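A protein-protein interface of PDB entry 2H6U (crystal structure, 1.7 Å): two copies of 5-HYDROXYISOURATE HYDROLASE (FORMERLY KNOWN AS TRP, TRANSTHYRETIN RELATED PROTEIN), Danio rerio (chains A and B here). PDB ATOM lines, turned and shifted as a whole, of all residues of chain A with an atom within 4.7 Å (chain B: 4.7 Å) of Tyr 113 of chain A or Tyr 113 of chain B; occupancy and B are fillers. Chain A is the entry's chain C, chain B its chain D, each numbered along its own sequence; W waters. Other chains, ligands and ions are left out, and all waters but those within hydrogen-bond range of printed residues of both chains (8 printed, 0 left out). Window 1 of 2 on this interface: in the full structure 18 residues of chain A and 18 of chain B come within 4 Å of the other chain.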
ATOM      1  N   TYR A  86     -23.607  -5.653  15.219  1.00  0.00           N
ATOM      2  CA  TYR A  86     -24.083  -4.444  14.530  1.00  0.00           C
ATOM      3  C   TYR A  86     -24.802  -3.534  15.529  1.00  0.00           C
ATOM      4  O   TYR A  86     -25.844  -3.919  16.059  1.00  0.00           O
ATOM      5  CB  TYR A  86     -25.050  -4.842  13.390  1.00  0.00           C
ATOM      6  CG  TYR A  86     -24.559  -6.043  12.590  1.00  0.00           C
ATOM      7  CD1 TYR A  86     -23.602  -5.899  11.590  1.00  0.00           C
ATOM      8  CD2 TYR A  86     -25.044  -7.324  12.853  1.00  0.00           C
ATOM      9  CE1 TYR A  86     -23.141  -7.002  10.863  1.00  0.00           C
ATOM     10  CE2 TYR A  86     -24.578  -8.433  12.166  1.00  0.00           C
ATOM     11  CZ  TYR A  86     -23.637  -8.273  11.155  1.00  0.00           C
ATOM     12  OH  TYR A  86     -23.176  -9.379  10.479  1.00  0.00           O
ATOM     13  N   VAL A  89     -28.725  -1.235  12.066  1.00  0.00           N
ATOM     14  CA  VAL A  89     -28.677  -1.645  10.671  1.00  0.00           C
ATOM     15  C   VAL A  89     -29.461  -0.640   9.836  1.00  0.00           C
ATOM     16  O   VAL A  89     -30.586  -0.283  10.190  1.00  0.00           O
ATOM     17  CB  VAL A  89     -29.324  -3.026  10.496  1.00  0.00           C
ATOM     18  CG1 VAL A  89     -29.447  -3.382   8.982  1.00  0.00           C
ATOM     19  CG2 VAL A  89     -28.530  -4.085  11.290  1.00  0.00           C
ATOM     20  N   GLU A  90     -28.874  -0.144   8.755  1.00  0.00           N
ATOM     21  CA  GLU A  90     -29.641   0.687   7.847  1.00  0.00           C
ATOM     22  C   GLU A  90     -29.758  -0.008   6.491  1.00  0.00           C
ATOM     23  O   GLU A  90     -28.754  -0.458   5.953  1.00  0.00           O
ATOM     24  CB  GLU A  90     -29.024   2.085   7.686  1.00  0.00           C
ATOM     25  CG  GLU A  90     -29.095   2.913   8.976  1.00  0.00           C
ATOM     26  CD  GLU A  90     -28.478   4.299   8.838  1.00  0.00           C
ATOM     27  OE1 GLU A  90     -27.525   4.451   8.041  1.00  0.00           O
ATOM     28  OE2 GLU A  90     -28.934   5.211   9.564  1.00  0.00           O
ATOM     29  N   ILE A  91     -30.978  -0.077   5.976  1.00  0.00           N
ATOM     30  CA  ILE A  91     -31.259  -0.581   4.631  1.00  0.00           C
ATOM     31  C   ILE A  91     -31.715   0.587   3.768  1.00  0.00           C
ATOM     32  O   ILE A  91     -32.713   1.266   4.079  1.00  0.00           O
ATOM     33  CB  ILE A  91     -32.352  -1.670   4.649  1.00  0.00           C
ATOM     34  CG1 ILE A  91     -31.943  -2.789   5.611  1.00  0.00           C
ATOM     35  CG2 ILE A  91     -32.605  -2.240   3.225  1.00  0.00           C
ATOM     36  CD1 ILE A  91     -33.033  -3.838   5.845  1.00  0.00           C
ATOM     37  N   LEU A 106     -36.286  -7.698   8.092  1.00  0.00           N
ATOM     38  CA  LEU A 106     -34.932  -7.880   8.615  1.00  0.00           C
ATOM     39  C   LEU A 106     -34.908  -9.220   9.303  1.00  0.00           C
ATOM     40  O   LEU A 106     -35.661  -9.424  10.252  1.00  0.00           O
ATOM     41  CB  LEU A 106     -34.572  -6.770   9.612  1.00  0.00           C
ATOM     42  CG  LEU A 106     -33.134  -6.846  10.153  1.00  0.00           C
ATOM     43  CD1 LEU A 106     -32.086  -6.606   9.058  1.00  0.00           C
ATOM     44  CD2 LEU A 106     -32.943  -5.865  11.311  1.00  0.00           C
ATOM     45  N   LEU A 107     -34.048 -10.128   8.838  1.00  0.00           N
ATOM     46  CA  LEU A 107     -33.860 -11.422   9.497  1.00  0.00           C
ATOM     47  C   LEU A 107     -32.564 -11.299  10.266  1.00  0.00           C
ATOM     48  O   LEU A 107     -31.519 -11.207   9.634  1.00  0.00           O
ATOM     49  CB  LEU A 107     -33.673 -12.539   8.443  1.00  0.00           C
ATOM     50  CG  LEU A 107     -34.860 -13.137   7.700  1.00  0.00           C
ATOM     51  CD1 LEU A 107     -35.855 -12.084   7.416  1.00  0.00           C
ATOM     52  CD2 LEU A 107     -34.432 -13.850   6.412  1.00  0.00           C
ATOM     53  N   LEU A 108     -32.608 -11.374  11.596  1.00  0.00           N
ATOM     54  CA  LEU A 108     -31.498 -10.946  12.454  1.00  0.00           C
ATOM     55  C   LEU A 108     -31.060 -11.978  13.496  1.00  0.00           C
ATOM     56  O   LEU A 108     -31.895 -12.604  14.131  1.00  0.00           O
ATOM     57  CB  LEU A 108     -31.972  -9.686  13.205  1.00  0.00           C
ATOM     58  CG  LEU A 108     -31.064  -9.027  14.236  1.00  0.00           C
ATOM     59  CD1 LEU A 108     -29.885  -8.367  13.484  1.00  0.00           C
ATOM     60  CD2 LEU A 108     -31.797  -8.023  15.085  1.00  0.00           C
ATOM     61  N   SER A 112     -25.459 -11.807  12.459  1.00  0.00           N
ATOM     62  CA  SER A 112     -25.837 -11.867  11.064  1.00  0.00           C
ATOM     63  C   SER A 112     -27.110 -11.087  10.830  1.00  0.00           C
ATOM     64  O   SER A 112     -27.899 -10.879  11.746  1.00  0.00           O
ATOM     65  CB  SER A 112     -26.100 -13.307  10.610  1.00  0.00           C
ATOM     66  OG  SER A 112     -27.278 -13.821  11.247  1.00  0.00           O
ATOM     67  N   TYR A 113     -27.298 -10.651   9.594  1.00  0.00           N
ATOM     68  CA  TYR A 113     -28.608 -10.213   9.174  1.00  0.00           C
ATOM     69  C   TYR A 113     -28.786 -10.336   7.671  1.00  0.00           C
ATOM     70  O   TYR A 113     -27.813 -10.466   6.911  1.00  0.00           O
ATOM     71  CB  TYR A 113     -28.911  -8.792   9.679  1.00  0.00           C
ATOM     72  CG  TYR A 113     -28.122  -7.659   9.036  1.00  0.00           C
ATOM     73  CD1 TYR A 113     -26.939  -7.194   9.620  1.00  0.00           C
ATOM     74  CD2 TYR A 113     -28.586  -7.027   7.877  1.00  0.00           C
ATOM     75  CE1 TYR A 113     -26.242  -6.142   9.079  1.00  0.00           C
ATOM     76  CE2 TYR A 113     -27.879  -5.963   7.312  1.00  0.00           C
ATOM     77  CZ  TYR A 113     -26.705  -5.530   7.933  1.00  0.00           C
ATOM     78  OH  TYR A 113     -25.980  -4.475   7.394  1.00  0.00           O
ATOM     79  N   SER A 114     -30.040 -10.331   7.239  1.00  0.00           N
ATOM     80  CA  SER A 114     -30.326 -10.425   5.823  1.00  0.00           C
ATOM     81  C   SER A 114     -31.646  -9.708   5.564  1.00  0.00           C
ATOM     82  O   SER A 114     -32.424  -9.459   6.480  1.00  0.00           O
ATOM     83  CB  SER A 114     -30.363 -11.880   5.335  1.00  0.00           C
ATOM     84  OG  SER A 114     -31.363 -12.631   5.996  1.00  0.00           O
ATOM     85  N   THR A 115     -31.847  -9.301   4.324  1.00  0.00           N
ATOM     86  CA  THR A 115     -33.062  -8.661   3.933  1.00  0.00           C
ATOM     87  C   THR A 115     -33.323  -9.029   2.478  1.00  0.00           C
ATOM     88  O   THR A 115     -32.436  -9.551   1.779  1.00  0.00           O
ATOM     89  CB  THR A 115     -32.959  -7.115   4.101  1.00  0.00           C
ATOM     90  OG1 THR A 115     -34.240  -6.528   3.894  1.00  0.00           O
ATOM     91  CG2 THR A 115     -31.993  -6.529   3.077  1.00  0.00           C
ATOM     92  N   TYR B  86     -31.049  -1.812  -4.041  1.00  0.00           N
ATOM     93  CA  TYR B  86     -30.255  -1.084  -3.049  1.00  0.00           C
ATOM     94  C   TYR B  86     -29.164  -0.308  -3.770  1.00  0.00           C
ATOM     95  O   TYR B  86     -28.306  -0.915  -4.399  1.00  0.00           O
ATOM     96  CB  TYR B  86     -29.612  -2.060  -2.056  1.00  0.00           C
ATOM     97  CG  TYR B  86     -30.570  -3.125  -1.555  1.00  0.00           C
ATOM     98  CD1 TYR B  86     -31.422  -2.879  -0.488  1.00  0.00           C
ATOM     99  CD2 TYR B  86     -30.610  -4.381  -2.166  1.00  0.00           C
ATOM    100  CE1 TYR B  86     -32.307  -3.871  -0.031  1.00  0.00           C
ATOM    101  CE2 TYR B  86     -31.479  -5.369  -1.721  1.00  0.00           C
ATOM    102  CZ  TYR B  86     -32.326  -5.107  -0.654  1.00  0.00           C
ATOM    103  OH  TYR B  86     -33.199  -6.086  -0.222  1.00  0.00           O
ATOM    104  N   VAL B  89     -24.908  -0.581  -0.062  1.00  0.00           N
ATOM    105  CA  VAL B  89     -25.115  -1.233   1.204  1.00  0.00           C
ATOM    106  C   VAL B  89     -24.029  -0.769   2.164  1.00  0.00           C
ATOM    107  O   VAL B  89     -22.852  -0.814   1.822  1.00  0.00           O
ATOM    108  CB  VAL B  89     -25.066  -2.763   1.075  1.00  0.00           C
ATOM    109  CG1 VAL B  89     -25.086  -3.424   2.469  1.00  0.00           C
ATOM    110  CG2 VAL B  89     -26.236  -3.275   0.211  1.00  0.00           C
ATOM    111  N   GLU B  90     -24.432  -0.364   3.369  1.00  0.00           N
ATOM    112  CA  GLU B  90     -23.465  -0.071   4.419  1.00  0.00           C
ATOM    113  C   GLU B  90     -23.666  -1.034   5.581  1.00  0.00           C
ATOM    114  O   GLU B  90     -24.786  -1.200   6.087  1.00  0.00           O
ATOM    115  CB  GLU B  90     -23.572   1.378   4.922  1.00  0.00           C
ATOM    116  CG  GLU B  90     -23.367   2.427   3.819  1.00  0.00           C
ATOM    117  CD  GLU B  90     -23.216   3.848   4.351  1.00  0.00           C
ATOM    118  OE1 GLU B  90     -24.028   4.273   5.203  1.00  0.00           O
ATOM    119  OE2 GLU B  90     -22.272   4.551   3.925  1.00  0.00           O
ATOM    120  N   ILE B  91     -22.573  -1.636   6.017  1.00  0.00           N
ATOM    121  CA  ILE B  91     -22.626  -2.520   7.164  1.00  0.00           C
ATOM    122  C   ILE B  91     -21.824  -1.867   8.286  1.00  0.00           C
ATOM    123  O   ILE B  91     -20.641  -1.560   8.107  1.00  0.00           O
ATOM    124  CB  ILE B  91     -22.047  -3.881   6.813  1.00  0.00           C
ATOM    125  CG1 ILE B  91     -22.827  -4.492   5.632  1.00  0.00           C
ATOM    126  CG2 ILE B  91     -22.020  -4.794   8.053  1.00  0.00           C
ATOM    127  CD1 ILE B  91     -22.218  -5.810   5.146  1.00  0.00           C
ATOM    128  N   LEU B 106     -20.468  -9.969   1.924  1.00  0.00           N
ATOM    129  CA  LEU B 106     -21.767  -9.566   1.402  1.00  0.00           C
ATOM    130  C   LEU B 106     -22.242 -10.571   0.372  1.00  0.00           C
ATOM    131  O   LEU B 106     -21.571 -10.793  -0.649  1.00  0.00           O
ATOM    132  CB  LEU B 106     -21.684  -8.193   0.773  1.00  0.00           C
ATOM    133  CG  LEU B 106     -22.993  -7.630   0.226  1.00  0.00           C
ATOM    134  CD1 LEU B 106     -23.951  -7.324   1.385  1.00  0.00           C
ATOM    135  CD2 LEU B 106     -22.746  -6.413  -0.616  1.00  0.00           C
ATOM    136  N   LEU B 107     -23.378 -11.215   0.654  1.00  0.00           N
ATOM    137  CA  LEU B 107     -24.039 -12.114  -0.306  1.00  0.00           C
ATOM    138  C   LEU B 107     -25.165 -11.330  -0.944  1.00  0.00           C
ATOM    139  O   LEU B 107     -26.055 -10.882  -0.236  1.00  0.00           O
ATOM    140  CB  LEU B 107     -24.613 -13.346   0.401  1.00  0.00           C
ATOM    141  CG  LEU B 107     -23.645 -14.342   1.025  1.00  0.00           C
ATOM    142  CD1 LEU B 107     -22.752 -13.688   2.055  1.00  0.00           C
ATOM    143  CD2 LEU B 107     -24.455 -15.467   1.681  1.00  0.00           C
ATOM    144  N   LEU B 108     -25.114 -11.144  -2.269  1.00  0.00           N
ATOM    145  CA  LEU B 108     -25.918 -10.136  -2.968  1.00  0.00           C
ATOM    146  C   LEU B 108     -26.669 -10.710  -4.164  1.00  0.00           C
ATOM    147  O   LEU B 108     -26.086 -11.466  -4.927  1.00  0.00           O
ATOM    148  CB  LEU B 108     -24.971  -9.020  -3.489  1.00  0.00           C
ATOM    149  CG  LEU B 108     -25.522  -7.769  -4.151  1.00  0.00           C
ATOM    150  CD1 LEU B 108     -26.439  -6.973  -3.177  1.00  0.00           C
ATOM    151  CD2 LEU B 108     -24.394  -6.885  -4.650  1.00  0.00           C
ATOM    152  N   SER B 112     -31.903  -8.683  -2.880  1.00  0.00           N
ATOM    153  CA  SER B 112     -31.650  -9.189  -1.523  1.00  0.00           C
ATOM    154  C   SER B 112     -30.168  -9.083  -1.148  1.00  0.00           C
ATOM    155  O   SER B 112     -29.311  -8.980  -2.019  1.00  0.00           O
ATOM    156  CB  SER B 112     -32.104 -10.645  -1.393  1.00  0.00           C
ATOM    157  OG  SER B 112     -31.134 -11.527  -1.949  1.00  0.00           O
ATOM    158  N   TYR B 113     -29.892  -9.053   0.148  1.00  0.00           N
ATOM    159  CA  TYR B 113     -28.512  -9.260   0.605  1.00  0.00           C
ATOM    160  C   TYR B 113     -28.456  -9.758   2.008  1.00  0.00           C
ATOM    161  O   TYR B 113     -29.417  -9.592   2.789  1.00  0.00           O
ATOM    162  CB  TYR B 113     -27.649  -8.008   0.435  1.00  0.00           C
ATOM    163  CG  TYR B 113     -27.967  -6.834   1.322  1.00  0.00           C
ATOM    164  CD1 TYR B 113     -28.809  -5.824   0.873  1.00  0.00           C
ATOM    165  CD2 TYR B 113     -27.363  -6.689   2.583  1.00  0.00           C
ATOM    166  CE1 TYR B 113     -29.095  -4.732   1.659  1.00  0.00           C
ATOM    167  CE2 TYR B 113     -27.639  -5.582   3.367  1.00  0.00           C
ATOM    168  CZ  TYR B 113     -28.493  -4.606   2.892  1.00  0.00           C
ATOM    169  OH  TYR B 113     -28.773  -3.495   3.674  1.00  0.00           O
ATOM    170  N   SER B 114     -27.312 -10.343   2.342  1.00  0.00           N
ATOM    171  CA  SER B 114     -27.095 -10.875   3.676  1.00  0.00           C
ATOM    172  C   SER B 114     -25.618 -10.754   4.040  1.00  0.00           C
ATOM    173  O   SER B 114     -24.752 -10.643   3.165  1.00  0.00           O
ATOM    174  CB  SER B 114     -27.580 -12.330   3.760  1.00  0.00           C
ATOM    175  OG  SER B 114     -26.586 -13.229   3.318  1.00  0.00           O
ATOM    176  N   THR B 115     -25.352 -10.743   5.335  1.00  0.00           N
ATOM    177  CA  THR B 115     -24.009 -10.633   5.843  1.00  0.00           C
ATOM    178  C   THR B 115     -23.991 -11.371   7.181  1.00  0.00           C
ATOM    179  O   THR B 115     -25.053 -11.647   7.767  1.00  0.00           O
ATOM    180  CB  THR B 115     -23.593  -9.156   6.032  1.00  0.00           C
ATOM    181  OG1 THR B 115     -22.207  -9.104   6.387  1.00  0.00           O
ATOM    182  CG2 THR B 115     -24.444  -8.452   7.153  1.00  0.00           C
HETATM  183  O   HOH W   1     -21.078  -8.889   8.854  1.00  0.00           O
HETATM  184  O   HOH W   2     -25.396   2.742   7.712  1.00  0.00           O
HETATM  185  O   HOH W   3     -27.078 -13.461   6.939  1.00  0.00           O
HETATM  186  O   HOH W   4     -26.870   3.346   5.049  1.00  0.00           O
HETATM  187  O   HOH W   5     -27.064  -2.828   5.684  1.00  0.00           O
HETATM  188  O   HOH W   6     -27.065   0.706   4.109  1.00  0.00           O
HETATM  189  O   HOH W   7     -35.037  -5.249   1.536  1.00  0.00           O
HETATM  190  O   HOH W   8     -25.993  -0.055   8.219  1.00  0.00           O
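Leu 107 of chain A touches none of the printed residues of chain B. Printed residues of chain B within 4 Å of Tyr 113 of chain A: Glu 90, Ile 91, Tyr 113, Ser 114 and Thr 115. Of the printed residues of chain B, Ser 114 of chain A touches Tyr 113 and Ser 114. Printed residues of chain A within 4 Å of Glu 90 of chain B: Tyr 113. Of the printed residues of chain A, Ile 91 of chain B touches Tyr 86 (3.7 Å) and Tyr 113 (3.6 Å). Of the printed residues of chain A, Tyr 113 of chain B touches Glu 90 (3.8 Å), Ile 91 (3.8 Å), Tyr 113 (3.97 Å), Ser 114 (3.3 Å) and Thr 115 (2.9 Å). Printed residues of chain A within 4 Å of Ser 114 of chain B: Tyr 113 (3.3 Å) and Ser 114 (3.2 Å). The nearest printed residue of chain A that does not touch Tyr 113 of chain B is Val 89 of chain A (5.4 Å).
Water W5 lies within hydrogen-bond range of the side-chain hydroxyl (OH) of Tyr 113 of chain A, the side-chain hydroxyl (OH) of Tyr 113 of chain B, the backbone carbonyl oxygen (O) of Glu 90 of chain B and the backbone carbonyl oxygen (O) of Glu 90 of chain A. Water W7 lies within hydrogen-bond range of OH of Tyr 86 of chain B (2.7 Å) and OG1 of Thr 115 of chain A (2.8 Å). Water W1 bridges OH of Tyr 86 of chain A (2.7 Å) and OG1 of Thr 115 of chain B (2.7 Å). Water W8 lies within hydrogen-bond range of O of Glu 90 of chain B (2.7 Å) and N of Glu 90 of chain A (2.9 Å). Water W2 bridges OE1 of Glu 90 of chain A (2.7 Å) and OE1 of Glu 90 of chain B (3.2 Å). Water W3 lies within hydrogen-bond range of O of Thr 115 of chain B (2.8 Å) and O of Tyr 113 of chain A (3.1 Å).
The backbone carbonyl oxygen of Tyr 113 of chain A is in hydrogen-bond range of the backbone NH of Thr 115 of chain B (2.9 Å). The backbone NH (N) of Thr 115 of chain A sits at hydrogen-bond distance from the backbone carbonyl oxygen (O) of Tyr 113 of chain B (2.9 Å).
Of the 11 printed residues of chain B, 7 touch a printed residue of chain A. Among the printed residues, no Asp or Glu carboxylate lies within 4 Å of a Lys or Arg side-chain nitrogen of the other chain.
O of Leu 107 of chain B lies within hydrogen-bond range of N of Ser 114 of chain B. N of Leu 107 of chain A is in hydrogen-bond range of O of Ser 114 of chain A (2.9 Å).
Among the printed residues, pairs that only touch across the chains: Tyr 86 of chain A with Ile 91 of chain B (3.7 Å), Tyr 86 of chain A with Thr 115 of chain B (3.7 Å), Glu 90 of chain A with Tyr 113 of chain B (3.8 Å), Ile 91 of chain A with Tyr 86 of chain B (3.7 Å), Ile 91 of chain A with Tyr 113 of chain B (3.8 Å), Ser 112 of chain A with Thr 115 of chain B (3.4 Å), Tyr 113 of chain A with Glu 90 of chain B (3.7 Å), Tyr 113 of chain A with Ile 91 of chain B (3.6 Å), Tyr 113 of chain A with Tyr 113 of chain B (3.97 Å), Tyr 113 of chain A with Ser 114 of chain B (3.3 Å), Ser 114 of chain A with Tyr 113 of chain B (3.3 Å), Ser 114 of chain A with Ser 114 of chain B (3.2 Å), Thr 115 of chain A with Tyr 86 of chain B (3.5 Å) and Thr 115 of chain A with Ser 112 of chain B (3.4 Å).
Tyr 86 of chain A touches Ile 91 of chain B, and with the chains exchanged Ile 91 of chain A touches Tyr 86 of chain B. Tyr 86 of chain A touches Thr 115 of chain B, and with the chains exchanged Thr 115 of chain A touches Tyr 86 of chain B. Ile 91 of chain A touches Tyr 113 of chain B, and with the chains exchanged Tyr 113 of chain A touches Ile 91 of chain B. Ser 112 of chain A touches Thr 115 of chain B, and with the chains exchanged Thr 115 of chain A touches Ser 112 of chain B. Of the 16 pairs that touch across the chains among the printed residues, 16 have their exchanged pair printed and touching as well.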
